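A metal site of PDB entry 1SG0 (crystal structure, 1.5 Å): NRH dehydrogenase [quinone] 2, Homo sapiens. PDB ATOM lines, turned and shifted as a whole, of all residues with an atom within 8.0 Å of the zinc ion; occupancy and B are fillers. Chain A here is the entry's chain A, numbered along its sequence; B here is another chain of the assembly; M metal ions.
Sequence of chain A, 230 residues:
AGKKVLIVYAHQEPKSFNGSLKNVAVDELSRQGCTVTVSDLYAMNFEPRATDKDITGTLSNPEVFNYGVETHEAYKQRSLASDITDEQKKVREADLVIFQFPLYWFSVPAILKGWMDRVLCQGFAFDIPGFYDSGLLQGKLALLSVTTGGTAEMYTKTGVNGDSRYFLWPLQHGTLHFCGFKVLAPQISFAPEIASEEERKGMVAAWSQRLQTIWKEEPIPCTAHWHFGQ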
ATOM      1  N   TYR A 132     -31.877 -15.764 -26.830  1.00  0.00           N
ATOM      2  CA  TYR A 132     -30.593 -15.203 -26.414  1.00  0.00           C
ATOM      3  C   TYR A 132     -29.512 -15.891 -27.257  1.00  0.00           C
ATOM      4  O   TYR A 132     -29.621 -15.924 -28.478  1.00  0.00           O
ATOM      5  CB  TYR A 132     -30.371 -15.379 -24.910  1.00  0.00           C
ATOM      6  CG  TYR A 132     -31.079 -14.307 -24.096  1.00  0.00           C
ATOM      7  CD1 TYR A 132     -30.864 -12.950 -24.368  1.00  0.00           C
ATOM      8  CD2 TYR A 132     -31.977 -14.636 -23.087  1.00  0.00           C
ATOM      9  CE1 TYR A 132     -31.523 -11.952 -23.655  1.00  0.00           C
ATOM     10  CE2 TYR A 132     -32.644 -13.638 -22.354  1.00  0.00           C
ATOM     11  CZ  TYR A 132     -32.414 -12.296 -22.648  1.00  0.00           C
ATOM     12  OH  TYR A 132     -33.060 -11.305 -21.936  1.00  0.00           O
ATOM     13  N   ASP A 133     -28.476 -16.432 -26.633  1.00  0.00           N
ATOM     14  CA  ASP A 133     -27.417 -17.087 -27.407  1.00  0.00           C
ATOM     15  C   ASP A 133     -27.945 -18.144 -28.383  1.00  0.00           C
ATOM     16  O   ASP A 133     -27.361 -18.362 -29.442  1.00  0.00           O
ATOM     17  CB  ASP A 133     -26.393 -17.712 -26.474  1.00  0.00           C
ATOM     18  CG  ASP A 133     -25.444 -16.686 -25.880  1.00  0.00           C
ATOM     19  OD1 ASP A 133     -25.932 -15.622 -25.448  1.00  0.00           O
ATOM     20  OD2 ASP A 133     -24.224 -16.952 -25.856  1.00  0.00           O
ATOM     21  N   TRP A 169     -30.102  -1.030 -23.510  1.00  0.00           N
ATOM     22  CA  TRP A 169     -30.484  -2.304 -22.914  1.00  0.00           C
ATOM     23  C   TRP A 169     -31.732  -2.980 -23.488  1.00  0.00           C
ATOM     24  O   TRP A 169     -31.675  -4.130 -23.936  1.00  0.00           O
ATOM     25  CB  TRP A 169     -30.637  -2.125 -21.392  1.00  0.00           C
ATOM     26  CG  TRP A 169     -31.013  -3.376 -20.627  1.00  0.00           C
ATOM     27  CD1 TRP A 169     -32.180  -3.599 -19.961  1.00  0.00           C
ATOM     28  CD2 TRP A 169     -30.184  -4.527 -20.385  1.00  0.00           C
ATOM     29  NE1 TRP A 169     -32.136  -4.813 -19.316  1.00  0.00           N
ATOM     30  CE2 TRP A 169     -30.930  -5.398 -19.563  1.00  0.00           C
ATOM     31  CE3 TRP A 169     -28.898  -4.897 -20.789  1.00  0.00           C
ATOM     32  CZ2 TRP A 169     -30.420  -6.638 -19.132  1.00  0.00           C
ATOM     33  CZ3 TRP A 169     -28.390  -6.127 -20.349  1.00  0.00           C
ATOM     34  CH2 TRP A 169     -29.150  -6.978 -19.531  1.00  0.00           C
ATOM     35  N   LEU A 171     -33.245  -2.510 -26.305  1.00  0.00           N
ATOM     36  CA  LEU A 171     -33.033  -2.782 -27.730  1.00  0.00           C
ATOM     37  C   LEU A 171     -31.976  -3.854 -28.001  1.00  0.00           C
ATOM     38  O   LEU A 171     -32.252  -4.825 -28.706  1.00  0.00           O
ATOM     39  CB  LEU A 171     -32.640  -1.482 -28.437  1.00  0.00           C
ATOM     40  CG  LEU A 171     -33.662  -0.351 -28.334  1.00  0.00           C
ATOM     41  CD1 LEU A 171     -33.079   0.916 -28.949  1.00  0.00           C
ATOM     42  CD2 LEU A 171     -34.961  -0.742 -29.026  1.00  0.00           C
ATOM     43  N   GLN A 172     -30.783  -3.667 -27.460  1.00  0.00           N
ATOM     44  CA  GLN A 172     -29.712  -4.618 -27.683  1.00  0.00           C
ATOM     45  C   GLN A 172     -29.882  -5.962 -26.977  1.00  0.00           C
ATOM     46  O   GLN A 172     -29.680  -7.009 -27.587  1.00  0.00           O
ATOM     47  CB  GLN A 172     -28.358  -4.010 -27.285  1.00  0.00           C
ATOM     48  CG  GLN A 172     -28.025  -2.718 -28.032  1.00  0.00           C
ATOM     49  CD  GLN A 172     -26.584  -2.276 -27.840  1.00  0.00           C
ATOM     50  OE1 GLN A 172     -26.017  -2.381 -26.749  1.00  0.00           O
ATOM     51  NE2 GLN A 172     -25.991  -1.750 -28.901  1.00  0.00           N
ATOM     52  N   HIS A 173     -30.274  -5.935 -25.707  1.00  0.00           N
ATOM     53  CA  HIS A 173     -30.426  -7.182 -24.956  1.00  0.00           C
ATOM     54  C   HIS A 173     -31.818  -7.797 -25.021  1.00  0.00           C
ATOM     55  O   HIS A 173     -31.979  -8.945 -25.438  1.00  0.00           O
ATOM     56  CB  HIS A 173     -30.048  -6.965 -23.491  1.00  0.00           C
ATOM     57  CG  HIS A 173     -30.037  -8.235 -22.692  1.00  0.00           C
ATOM     58  ND1 HIS A 173     -29.013  -9.158 -22.756  1.00  0.00           N
ATOM     59  CD2 HIS A 173     -30.940  -8.742 -21.818  1.00  0.00           C
ATOM     60  CE1 HIS A 173     -29.289 -10.181 -21.965  1.00  0.00           C
ATOM     61  NE2 HIS A 173     -30.451  -9.961 -21.384  1.00  0.00           N
ATOM     62  N   GLY A 174     -32.813  -7.035 -24.585  1.00  0.00           N
ATOM     63  CA  GLY A 174     -34.174  -7.544 -24.568  1.00  0.00           C
ATOM     64  C   GLY A 174     -34.744  -7.912 -25.917  1.00  0.00           C
ATOM     65  O   GLY A 174     -35.639  -8.749 -26.007  1.00  0.00           O
ATOM     66  N   THR A 175     -34.223  -7.293 -26.976  1.00  0.00           N
ATOM     67  CA  THR A 175     -34.738  -7.566 -28.314  1.00  0.00           C
ATOM     68  C   THR A 175     -33.756  -8.307 -29.220  1.00  0.00           C
ATOM     69  O   THR A 175     -33.981  -9.475 -29.536  1.00  0.00           O
ATOM     70  CB  THR A 175     -35.151  -6.248 -29.014  1.00  0.00           C
ATOM     71  OG1 THR A 175     -36.024  -5.508 -28.160  1.00  0.00           O
ATOM     72  CG2 THR A 175     -35.865  -6.542 -30.310  1.00  0.00           C
ATOM     73  N   LEU A 176     -32.679  -7.642 -29.624  1.00  0.00           N
ATOM     74  CA  LEU A 176     -31.708  -8.230 -30.529  1.00  0.00           C
ATOM     75  C   LEU A 176     -31.004  -9.481 -30.009  1.00  0.00           C
ATOM     76  O   LEU A 176     -31.015 -10.526 -30.667  1.00  0.00           O
ATOM     77  CB  LEU A 176     -30.688  -7.172 -30.950  1.00  0.00           C
ATOM     78  CG  LEU A 176     -31.293  -5.940 -31.638  1.00  0.00           C
ATOM     79  CD1 LEU A 176     -30.216  -4.901 -31.858  1.00  0.00           C
ATOM     80  CD2 LEU A 176     -31.936  -6.344 -32.961  1.00  0.00           C
ATOM     81  N   HIS A 177     -30.392  -9.389 -28.822  1.00  0.00           N
ATOM     82  CA  HIS A 177     -29.701 -10.540 -28.259  1.00  0.00           C
ATOM     83  C   HIS A 177     -30.690 -11.673 -28.013  1.00  0.00           C
ATOM     84  O   HIS A 177     -30.388 -12.848 -28.249  1.00  0.00           O
ATOM     85  CB  HIS A 177     -29.018 -10.167 -26.932  1.00  0.00           C
ATOM     86  CG  HIS A 177     -28.121 -11.238 -26.381  1.00  0.00           C
ATOM     87  ND1 HIS A 177     -27.498 -11.123 -25.161  1.00  0.00           N
ATOM     88  CD2 HIS A 177     -27.741 -12.438 -26.889  1.00  0.00           C
ATOM     89  CE1 HIS A 177     -26.767 -12.200 -24.935  1.00  0.00           C
ATOM     90  NE2 HIS A 177     -26.899 -13.014 -25.974  1.00  0.00           N
ATOM     91  N   PHE A 178     -31.895 -11.331 -27.551  1.00  0.00           N
ATOM     92  CA  PHE A 178     -32.897 -12.349 -27.281  1.00  0.00           C
ATOM     93  C   PHE A 178     -33.184 -13.182 -28.533  1.00  0.00           C
ATOM     94  O   PHE A 178     -33.432 -14.378 -28.439  1.00  0.00           O
ATOM     95  CB  PHE A 178     -34.195 -11.705 -26.788  1.00  0.00           C
ATOM     96  CG  PHE A 178     -35.236 -12.709 -26.361  1.00  0.00           C
ATOM     97  CD1 PHE A 178     -35.151 -13.326 -25.109  1.00  0.00           C
ATOM     98  CD2 PHE A 178     -36.292 -13.038 -27.194  1.00  0.00           C
ATOM     99  CE1 PHE A 178     -36.099 -14.269 -24.710  1.00  0.00           C
ATOM    100  CE2 PHE A 178     -37.248 -13.984 -26.818  1.00  0.00           C
ATOM    101  CZ  PHE A 178     -37.147 -14.598 -25.565  1.00  0.00           C
ATOM    102  N   PHE A 181     -29.243 -12.430 -32.296  1.00  0.00           N
ATOM    103  CA  PHE A 181     -28.365 -11.520 -33.004  1.00  0.00           C
ATOM    104  C   PHE A 181     -27.046 -11.294 -32.271  1.00  0.00           C
ATOM    105  O   PHE A 181     -27.015 -11.177 -31.049  1.00  0.00           O
ATOM    106  CB  PHE A 181     -29.021 -10.154 -33.160  1.00  0.00           C
ATOM    107  CG  PHE A 181     -29.970 -10.037 -34.322  1.00  0.00           C
ATOM    108  CD1 PHE A 181     -29.494 -10.021 -35.624  1.00  0.00           C
ATOM    109  CD2 PHE A 181     -31.332  -9.889 -34.107  1.00  0.00           C
ATOM    110  CE1 PHE A 181     -30.359  -9.849 -36.694  1.00  0.00           C
ATOM    111  CE2 PHE A 181     -32.214  -9.719 -35.178  1.00  0.00           C
ATOM    112  CZ  PHE A 181     -31.716  -9.692 -36.477  1.00  0.00           C
ATOM    113  N   VAL A 183     -24.598  -8.684 -31.503  1.00  0.00           N
ATOM    114  CA  VAL A 183     -24.727  -7.233 -31.523  1.00  0.00           C
ATOM    115  C   VAL A 183     -23.434  -6.458 -31.698  1.00  0.00           C
ATOM    116  O   VAL A 183     -22.554  -6.498 -30.837  1.00  0.00           O
ATOM    117  CB  VAL A 183     -25.424  -6.740 -30.230  1.00  0.00           C
ATOM    118  CG1 VAL A 183     -25.699  -5.248 -30.316  1.00  0.00           C
ATOM    119  CG2 VAL A 183     -26.714  -7.510 -30.025  1.00  0.00           C
ATOM    120  N   ILE A 220     -20.192  -7.180 -29.477  1.00  0.00           N
ATOM    121  CA  ILE A 220     -19.951  -6.729 -28.114  1.00  0.00           C
ATOM    122  C   ILE A 220     -20.494  -7.783 -27.157  1.00  0.00           C
ATOM    123  O   ILE A 220     -21.310  -8.628 -27.552  1.00  0.00           O
ATOM    124  CB  ILE A 220     -20.713  -5.417 -27.790  1.00  0.00           C
ATOM    125  CG1 ILE A 220     -22.217  -5.689 -27.811  1.00  0.00           C
ATOM    126  CG2 ILE A 220     -20.340  -4.336 -28.803  1.00  0.00           C
ATOM    127  CD1 ILE A 220     -23.065  -4.539 -27.294  1.00  0.00           C
ATOM    128  N   PRO A 221     -20.020  -7.779 -25.905  1.00  0.00           N
ATOM    129  CA  PRO A 221     -20.520  -8.765 -24.942  1.00  0.00           C
ATOM    130  C   PRO A 221     -21.831  -8.178 -24.415  1.00  0.00           C
ATOM    131  O   PRO A 221     -21.827  -7.410 -23.455  1.00  0.00           O
ATOM    132  CB  PRO A 221     -19.416  -8.804 -23.896  1.00  0.00           C
ATOM    133  CG  PRO A 221     -18.920  -7.401 -23.887  1.00  0.00           C
ATOM    134  CD  PRO A 221     -18.865  -7.052 -25.364  1.00  0.00           C
ATOM    135  N   CYS A 222     -22.934  -8.528 -25.061  1.00  0.00           N
ATOM    136  CA  CYS A 222     -24.243  -7.996 -24.670  1.00  0.00           C
ATOM    137  C   CYS A 222     -24.694  -8.533 -23.315  1.00  0.00           C
ATOM    138  O   CYS A 222     -25.562  -9.403 -23.231  1.00  0.00           O
ATOM    139  CB  CYS A 222     -25.280  -8.327 -25.739  1.00  0.00           C
ATOM    140  SG  CYS A 222     -26.823  -7.404 -25.547  1.00  0.00           S
ATOM    141  N   THR A 223     -24.101  -7.998 -22.263  1.00  0.00           N
ATOM    142  CA  THR A 223     -24.416  -8.421 -20.912  1.00  0.00           C
ATOM    143  C   THR A 223     -24.811  -7.232 -20.049  1.00  0.00           C
ATOM    144  O   THR A 223     -24.559  -6.084 -20.393  1.00  0.00           O
ATOM    145  CB  THR A 223     -23.199  -9.092 -20.262  1.00  0.00           C
ATOM    146  OG1 THR A 223     -22.103  -8.182 -20.256  1.00  0.00           O
ATOM    147  CG2 THR A 223     -22.819 -10.349 -21.022  1.00  0.00           C
ATOM    148  N   ALA A 224     -25.427  -7.522 -18.910  1.00  0.00           N
ATOM    149  CA  ALA A 224     -25.834  -6.485 -17.984  1.00  0.00           C
ATOM    150  C   ALA A 224     -24.604  -5.682 -17.564  1.00  0.00           C
ATOM    151  O   ALA A 224     -24.675  -4.473 -17.344  1.00  0.00           O
ATOM    152  CB  ALA A 224     -26.508  -7.101 -16.762  1.00  0.00           C
ATOM    153  N   TRP A 226     -21.859  -5.050 -19.380  1.00  0.00           N
ATOM    154  CA  TRP A 226     -21.460  -4.152 -20.455  1.00  0.00           C
ATOM    155  C   TRP A 226     -22.304  -2.883 -20.422  1.00  0.00           C
ATOM    156  O   TRP A 226     -21.786  -1.777 -20.585  1.00  0.00           O
ATOM    157  CB  TRP A 226     -21.637  -4.840 -21.814  1.00  0.00           C
ATOM    158  CG  TRP A 226     -21.134  -4.015 -22.965  1.00  0.00           C
ATOM    159  CD1 TRP A 226     -19.864  -4.005 -23.484  1.00  0.00           C
ATOM    160  CD2 TRP A 226     -21.873  -3.066 -23.725  1.00  0.00           C
ATOM    161  NE1 TRP A 226     -19.773  -3.108 -24.513  1.00  0.00           N
ATOM    162  CE2 TRP A 226     -20.995  -2.510 -24.680  1.00  0.00           C
ATOM    163  CE3 TRP A 226     -23.202  -2.609 -23.684  1.00  0.00           C
ATOM    164  CZ2 TRP A 226     -21.399  -1.531 -25.596  1.00  0.00           C
ATOM    165  CZ3 TRP A 226     -23.606  -1.631 -24.599  1.00  0.00           C
ATOM    166  CH2 TRP A 226     -22.701  -1.102 -25.535  1.00  0.00           C
ATOM    167  N   HIS A 227     -23.601  -3.049 -20.221  1.00  0.00           N
ATOM    168  CA  HIS A 227     -24.519  -1.913 -20.190  1.00  0.00           C
ATOM    169  C   HIS A 227     -24.518  -1.102 -18.894  1.00  0.00           C
ATOM    170  O   HIS A 227     -24.636   0.120 -18.934  1.00  0.00           O
ATOM    171  CB  HIS A 227     -25.959  -2.367 -20.449  1.00  0.00           C
ATOM    172  CG  HIS A 227     -26.207  -2.878 -21.842  1.00  0.00           C
ATOM    173  ND1 HIS A 227     -25.799  -4.120 -22.255  1.00  0.00           N
ATOM    174  CD2 HIS A 227     -26.822  -2.301 -22.895  1.00  0.00           C
ATOM    175  CE1 HIS A 227     -26.159  -4.292 -23.519  1.00  0.00           C
ATOM    176  NE2 HIS A 227     -26.783  -3.202 -23.929  1.00  0.00           N
ATOM    177  N   VAL B 160     -31.307 -13.886 -16.284  1.00  0.00           N
ATOM    178  CA  VAL B 160     -31.065 -13.797 -17.717  1.00  0.00           C
ATOM    179  C   VAL B 160     -31.595 -12.511 -18.351  1.00  0.00           C
ATOM    180  O   VAL B 160     -31.073 -12.049 -19.361  1.00  0.00           O
ATOM    181  CB  VAL B 160     -31.678 -15.015 -18.443  1.00  0.00           C
ATOM    182  CG1 VAL B 160     -33.195 -14.969 -18.359  1.00  0.00           C
ATOM    183  CG2 VAL B 160     -31.210 -15.074 -19.871  1.00  0.00           C
HETATM  184 ZN    ZN M   1     -27.455  -9.203 -24.227  1.00  0.00          ZN
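The zinc ion is bound by a ring nitrogen (ND1) of His 177, at 2.1 Å.
A ring nitrogen (ND1) of His 173 is bound to the zinc ion (2.1 Å).
The backbone carbonyl oxygen (O) of Cys 222 is bound to the zinc ion (2.1 Å).
The zinc ion is bound by the side-chain sulfur (SG) of Cys 222 (2.3 Å).
A ring nitrogen (NE2) of His 177 is in hydrogen-bond range of the side-chain carboxylate of Asp 133.
The side-chain sulfur (SG) of Cys 222 sits close to the backbone carbonyl oxygen (O) of Gln 172, 3.5 Å away.
The side-chain hydroxyl of Tyr 132 lies within hydrogen-bond range of a ring nitrogen (NE2) of His 173 (3.0 Å).
O of Gln 172 lies within hydrogen-bond range of N of His 177 (2.8 Å).
NE2 of His 173 lies within hydrogen-bond range of O of Val 160 of chain B, 3.0 Å away.
O of His 173 lies within hydrogen-bond range of N of Phe 178, at 3.2 Å.
Of the 21 residues printed, 3 come within 4 Å of the zinc ion.
The nearest printed residue that does not touch the zinc ion is Thr 223 (4.1 Å).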
